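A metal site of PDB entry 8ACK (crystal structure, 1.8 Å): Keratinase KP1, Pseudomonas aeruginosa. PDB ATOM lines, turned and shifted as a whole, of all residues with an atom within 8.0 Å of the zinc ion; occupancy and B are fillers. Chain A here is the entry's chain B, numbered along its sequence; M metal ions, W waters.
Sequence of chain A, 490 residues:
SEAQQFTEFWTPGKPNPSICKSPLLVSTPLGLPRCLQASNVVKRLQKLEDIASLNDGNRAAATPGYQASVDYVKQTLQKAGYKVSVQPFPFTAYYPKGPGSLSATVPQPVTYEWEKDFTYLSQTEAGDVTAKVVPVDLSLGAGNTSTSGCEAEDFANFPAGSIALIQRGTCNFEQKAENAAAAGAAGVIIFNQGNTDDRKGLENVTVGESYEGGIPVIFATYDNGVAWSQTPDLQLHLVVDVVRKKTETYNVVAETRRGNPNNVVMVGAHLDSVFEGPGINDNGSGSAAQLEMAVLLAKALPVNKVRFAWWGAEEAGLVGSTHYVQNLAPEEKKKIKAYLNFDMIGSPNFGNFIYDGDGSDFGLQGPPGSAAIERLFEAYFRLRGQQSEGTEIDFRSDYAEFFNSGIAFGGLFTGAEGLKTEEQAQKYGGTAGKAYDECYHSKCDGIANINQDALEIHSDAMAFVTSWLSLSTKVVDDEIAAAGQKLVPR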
ATOM      1  N   ILE A 354      14.097 -18.528  -4.825  1.00  0.00           N
ATOM      2  CA  ILE A 354      12.928 -17.951  -5.462  1.00  0.00           C
ATOM      3  C   ILE A 354      12.870 -16.475  -5.104  1.00  0.00           C
ATOM      4  O   ILE A 354      13.071 -16.114  -3.933  1.00  0.00           O
ATOM      5  CB  ILE A 354      11.628 -18.670  -5.027  1.00  0.00           C
ATOM      6  CG1 ILE A 354      11.696 -20.170  -5.364  1.00  0.00           C
ATOM      7  CG2 ILE A 354      10.424 -18.024  -5.684  1.00  0.00           C
ATOM      8  CD1 ILE A 354      10.578 -21.007  -4.657  1.00  0.00           C
ATOM      9  N   TYR A 355      12.636 -15.617  -6.090  1.00  0.00           N
ATOM     10  CA  TYR A 355      12.562 -14.184  -5.813  1.00  0.00           C
ATOM     11  C   TYR A 355      11.564 -13.919  -4.710  1.00  0.00           C
ATOM     12  O   TYR A 355      10.418 -14.388  -4.763  1.00  0.00           O
ATOM     13  CB  TYR A 355      12.152 -13.398  -7.057  1.00  0.00           C
ATOM     14  CG  TYR A 355      13.191 -13.278  -8.141  1.00  0.00           C
ATOM     15  CD1 TYR A 355      14.382 -13.997  -8.110  1.00  0.00           C
ATOM     16  CD2 TYR A 355      12.961 -12.434  -9.220  1.00  0.00           C
ATOM     17  CE1 TYR A 355      15.319 -13.866  -9.137  1.00  0.00           C
ATOM     18  CE2 TYR A 355      13.882 -12.295 -10.231  1.00  0.00           C
ATOM     19  CZ  TYR A 355      15.052 -13.010 -10.192  1.00  0.00           C
ATOM     20  OH  TYR A 355      15.935 -12.853 -11.231  1.00  0.00           O
ATOM     21  N   ASP A 356      11.982 -13.116  -3.715  1.00  0.00           N
ATOM     22  CA  ASP A 356      11.178 -12.850  -2.510  1.00  0.00           C
ATOM     23  C   ASP A 356      10.152 -11.747  -2.784  1.00  0.00           C
ATOM     24  O   ASP A 356      10.149 -10.675  -2.160  1.00  0.00           O
ATOM     25  CB  ASP A 356      12.074 -12.505  -1.331  1.00  0.00           C
ATOM     26  CG  ASP A 356      11.285 -12.215  -0.073  1.00  0.00           C
ATOM     27  OD1 ASP A 356      10.259 -12.901   0.156  1.00  0.00           O
ATOM     28  OD2 ASP A 356      11.669 -11.303   0.681  1.00  0.00           O
ATOM     29  N   GLY A 357       9.213 -12.054  -3.676  1.00  0.00           N
ATOM     30  CA  GLY A 357       8.198 -11.098  -4.074  1.00  0.00           C
ATOM     31  C   GLY A 357       7.344 -10.575  -2.935  1.00  0.00           C
ATOM     32  O   GLY A 357       6.919  -9.411  -2.971  1.00  0.00           O
ATOM     33  N   ASP A 358       7.058 -11.402  -1.930  1.00  0.00           N
ATOM     34  CA  ASP A 358       6.222 -10.958  -0.819  1.00  0.00           C
ATOM     35  C   ASP A 358       7.006 -10.202   0.255  1.00  0.00           C
ATOM     36  O   ASP A 358       6.401  -9.730   1.222  1.00  0.00           O
ATOM     37  CB  ASP A 358       5.453 -12.136  -0.177  1.00  0.00           C
ATOM     38  CG  ASP A 358       6.379 -13.230   0.378  1.00  0.00           C
ATOM     39  OD1 ASP A 358       7.613 -13.138   0.256  1.00  0.00           O
ATOM     40  OD2 ASP A 358       5.844 -14.226   0.915  1.00  0.00           O
ATOM     41  N   GLY A 359       8.315 -10.050   0.088  1.00  0.00           N
ATOM     42  CA  GLY A 359       9.104  -9.360   1.083  1.00  0.00           C
ATOM     43  C   GLY A 359       9.198 -10.088   2.403  1.00  0.00           C
ATOM     44  O   GLY A 359       9.647  -9.493   3.385  1.00  0.00           O
ATOM     45  N   SER A 360       8.785 -11.359   2.457  1.00  0.00           N
ATOM     46  CA  SER A 360       8.768 -12.076   3.728  1.00  0.00           C
ATOM     47  C   SER A 360      10.161 -12.294   4.292  1.00  0.00           C
ATOM     48  O   SER A 360      10.303 -12.496   5.502  1.00  0.00           O
ATOM     49  CB  SER A 360       8.061 -13.425   3.549  1.00  0.00           C
ATOM     50  OG  SER A 360       8.779 -14.224   2.616  1.00  0.00           O
ATOM     51  N   ASP A 361      11.194 -12.302   3.455  1.00  0.00           N
ATOM     52  CA  ASP A 361      12.549 -12.507   3.932  1.00  0.00           C
ATOM     53  C   ASP A 361      13.339 -11.211   4.061  1.00  0.00           C
ATOM     54  O   ASP A 361      13.993 -11.002   5.076  1.00  0.00           O
ATOM     55  CB  ASP A 361      13.313 -13.463   3.012  1.00  0.00           C
ATOM     56  CG  ASP A 361      12.690 -14.849   2.960  1.00  0.00           C
ATOM     57  OD1 ASP A 361      12.077 -15.275   3.961  1.00  0.00           O
ATOM     58  OD2 ASP A 361      12.835 -15.518   1.920  1.00  0.00           O
ATOM     59  N   PHE A 362      13.244 -10.318   3.075  1.00  0.00           N
ATOM     60  CA  PHE A 362      14.105  -9.146   3.012  1.00  0.00           C
ATOM     61  C   PHE A 362      13.341  -7.821   3.046  1.00  0.00           C
ATOM     62  O   PHE A 362      13.961  -6.768   2.958  1.00  0.00           O
ATOM     63  CB  PHE A 362      14.988  -9.199   1.764  1.00  0.00           C
ATOM     64  CG  PHE A 362      15.693 -10.507   1.576  1.00  0.00           C
ATOM     65  CD1 PHE A 362      16.842 -10.811   2.310  1.00  0.00           C
ATOM     66  CD2 PHE A 362      15.199 -11.466   0.691  1.00  0.00           C
ATOM     67  CE1 PHE A 362      17.487 -12.024   2.150  1.00  0.00           C
ATOM     68  CE2 PHE A 362      15.844 -12.679   0.531  1.00  0.00           C
ATOM     69  CZ  PHE A 362      16.984 -12.966   1.261  1.00  0.00           C
ATOM     70  N   GLY A 363      12.008  -7.858   3.175  1.00  0.00           N
ATOM     71  CA  GLY A 363      11.254  -6.656   3.446  1.00  0.00           C
ATOM     72  C   GLY A 363      10.969  -5.770   2.248  1.00  0.00           C
ATOM     73  O   GLY A 363      10.377  -4.699   2.421  1.00  0.00           O
ATOM     74  N   LEU A 364      11.353  -6.169   1.040  1.00  0.00           N
ATOM     75  CA  LEU A 364      11.007  -5.447  -0.176  1.00  0.00           C
ATOM     76  C   LEU A 364       9.941  -6.240  -0.926  1.00  0.00           C
ATOM     77  O   LEU A 364      10.178  -7.391  -1.313  1.00  0.00           O
ATOM     78  CB  LEU A 364      12.228  -5.220  -1.049  1.00  0.00           C
ATOM     79  CG  LEU A 364      12.006  -4.436  -2.348  1.00  0.00           C
ATOM     80  CD1 LEU A 364      11.318  -3.111  -2.090  1.00  0.00           C
ATOM     81  CD2 LEU A 364      13.336  -4.218  -3.084  1.00  0.00           C
ATOM     82  N   SER A 370       3.221 -10.075  -7.449  1.00  0.00           N
ATOM     83  CA  SER A 370       4.525 -10.709  -7.285  1.00  0.00           C
ATOM     84  C   SER A 370       4.488 -11.776  -6.187  1.00  0.00           C
ATOM     85  O   SER A 370       5.189 -12.786  -6.262  1.00  0.00           O
ATOM     86  CB  SER A 370       5.578  -9.648  -6.985  1.00  0.00           C
ATOM     87  OG  SER A 370       5.539  -8.622  -7.973  1.00  0.00           O
ATOM     88  N   ALA A 371       3.708 -11.540  -5.127  1.00  0.00           N
ATOM     89  CA  ALA A 371       3.554 -12.561  -4.108  1.00  0.00           C
ATOM     90  C   ALA A 371       2.951 -13.829  -4.706  1.00  0.00           C
ATOM     91  O   ALA A 371       3.381 -14.947  -4.400  1.00  0.00           O
ATOM     92  CB  ALA A 371       2.701 -12.045  -2.953  1.00  0.00           C
ATOM     93  N   GLU A 374       5.628 -15.725  -6.697  1.00  0.00           N
ATOM     94  CA  GLU A 374       6.512 -16.396  -5.767  1.00  0.00           C
ATOM     95  C   GLU A 374       5.838 -17.626  -5.156  1.00  0.00           C
ATOM     96  O   GLU A 374       6.457 -18.700  -5.068  1.00  0.00           O
ATOM     97  CB  GLU A 374       6.939 -15.430  -4.665  1.00  0.00           C
ATOM     98  CG  GLU A 374       7.667 -16.109  -3.527  1.00  0.00           C
ATOM     99  CD  GLU A 374       7.976 -15.177  -2.374  1.00  0.00           C
ATOM    100  OE1 GLU A 374       7.159 -14.285  -2.064  1.00  0.00           O
ATOM    101  OE2 GLU A 374       9.065 -15.315  -1.799  1.00  0.00           O
ATOM    102  N   ARG A 375       4.564 -17.494  -4.787  1.00  0.00           N
ATOM    103  CA  ARG A 375       3.812 -18.609  -4.201  1.00  0.00           C
ATOM    104  C   ARG A 375       3.647 -19.775  -5.175  1.00  0.00           C
ATOM    105  O   ARG A 375       3.643 -20.942  -4.760  1.00  0.00           O
ATOM    106  CB  ARG A 375       2.449 -18.099  -3.733  1.00  0.00           C
ATOM    107  CG  ARG A 375       1.755 -18.923  -2.686  1.00  0.00           C
ATOM    108  CD  ARG A 375       0.527 -18.165  -2.197  1.00  0.00           C
ATOM    109  NE  ARG A 375       0.921 -16.942  -1.506  1.00  0.00           N
ATOM    110  CZ  ARG A 375       0.633 -15.700  -1.914  1.00  0.00           C
ATOM    111  NH1 ARG A 375      -0.075 -15.515  -3.029  1.00  0.00           N
ATOM    112  NH2 ARG A 375       1.036 -14.663  -1.201  1.00  0.00           N
ATOM    113  N   GLU A 378       6.961 -21.513  -5.144  1.00  0.00           N
ATOM    114  CA  GLU A 378       7.131 -22.187  -3.853  1.00  0.00           C
ATOM    115  C   GLU A 378       6.359 -23.493  -3.812  1.00  0.00           C
ATOM    116  O   GLU A 378       6.866 -24.515  -3.347  1.00  0.00           O
ATOM    117  CB  GLU A 378       6.669 -21.285  -2.694  1.00  0.00           C
ATOM    118  CG  GLU A 378       7.600 -20.106  -2.373  1.00  0.00           C
ATOM    119  CD  GLU A 378       6.988 -19.148  -1.356  1.00  0.00           C
ATOM    120  OE1 GLU A 378       7.713 -18.268  -0.831  1.00  0.00           O
ATOM    121  OE2 GLU A 378       5.778 -19.272  -1.067  1.00  0.00           O
ATOM    122  N   GLU A 389      14.165 -21.365  -0.911  1.00  0.00           N
ATOM    123  CA  GLU A 389      14.155 -20.227  -0.008  1.00  0.00           C
ATOM    124  C   GLU A 389      14.274 -18.932  -0.823  1.00  0.00           C
ATOM    125  O   GLU A 389      14.523 -18.949  -2.034  1.00  0.00           O
ATOM    126  CB  GLU A 389      15.280 -20.329   1.026  1.00  0.00           C
ATOM    127  CG  GLU A 389      16.669 -20.251   0.424  1.00  0.00           C
ATOM    128  CD  GLU A 389      17.740 -20.622   1.421  1.00  0.00           C
ATOM    129  OE1 GLU A 389      18.025 -21.834   1.577  1.00  0.00           O
ATOM    130  OE2 GLU A 389      18.306 -19.696   2.063  1.00  0.00           O
ATOM    131  N   GLY A 390      14.091 -17.817  -0.132  1.00  0.00           N
ATOM    132  CA  GLY A 390      13.995 -16.552  -0.835  1.00  0.00           C
ATOM    133  C   GLY A 390      15.349 -15.957  -1.192  1.00  0.00           C
ATOM    134  O   GLY A 390      16.386 -16.282  -0.615  1.00  0.00           O
ATOM    135  N   THR A 391      15.327 -15.075  -2.185  1.00  0.00           N
ATOM    136  CA  THR A 391      16.487 -14.274  -2.531  1.00  0.00           C
ATOM    137  C   THR A 391      16.019 -12.841  -2.804  1.00  0.00           C
ATOM    138  O   THR A 391      14.848 -12.607  -3.103  1.00  0.00           O
ATOM    139  CB  THR A 391      17.257 -14.864  -3.716  1.00  0.00           C
ATOM    140  OG1 THR A 391      18.470 -14.123  -3.920  1.00  0.00           O
ATOM    141  CG2 THR A 391      16.426 -14.835  -4.995  1.00  0.00           C
HETATM  142 ZN    ZN M   1       9.009 -14.532   0.316  1.00  0.00          ZN
HETATM  143  O   HOH W   1       7.454 -16.176   0.960  1.00  0.00           O
HETATM  144  O   HOH W   2      10.525 -15.768   0.590  1.00  0.00           O
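The zinc ion is bound by OD1 of Asp 358, 2.0 Å away.
Water W2 is bound to the zinc ion (2.0 Å).
OD1 of Asp 356 binds the zinc ion (2.1 Å).
The zinc ion is bound by the side-chain carboxylate (OE2) of Glu 374 (2.3 Å).
The zinc ion is bound by the side-chain hydroxyl (OG) of Ser 360, 2.3 Å away.
Water W1 is bound to the zinc ion.
Water W1 bridges the side-chain carboxylate of Asp 358 (2.5 Å) and the side-chain carboxylate of Glu 378 (2.8 Å).
The backbone NH of Asp 361 is in hydrogen-bond range of the side-chain carboxylate of Asp 356 (3.0 Å).
The side-chain carboxylate of Asp 356 sits close to the backbone NH of Gly 359.
The side-chain carboxylate of Asp 356 is in hydrogen-bond range of the backbone NH of Phe 362 (3.0 Å).
The backbone NH (N) of Asp 356 is in hydrogen-bond range of the backbone carbonyl oxygen (O) of Thr 391 (3.0 Å).
The backbone NH (N) of Gly 357 lies within hydrogen-bond range of the side-chain carboxylate (OE1) of Glu 374, 3.4 Å away.
Within 4 Å of the zinc ion: Asp 356, Asp 358, Ser 360 and Glu 374.
The nearest printed residue that does not touch the zinc ion is Glu 378 (4.1 Å).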
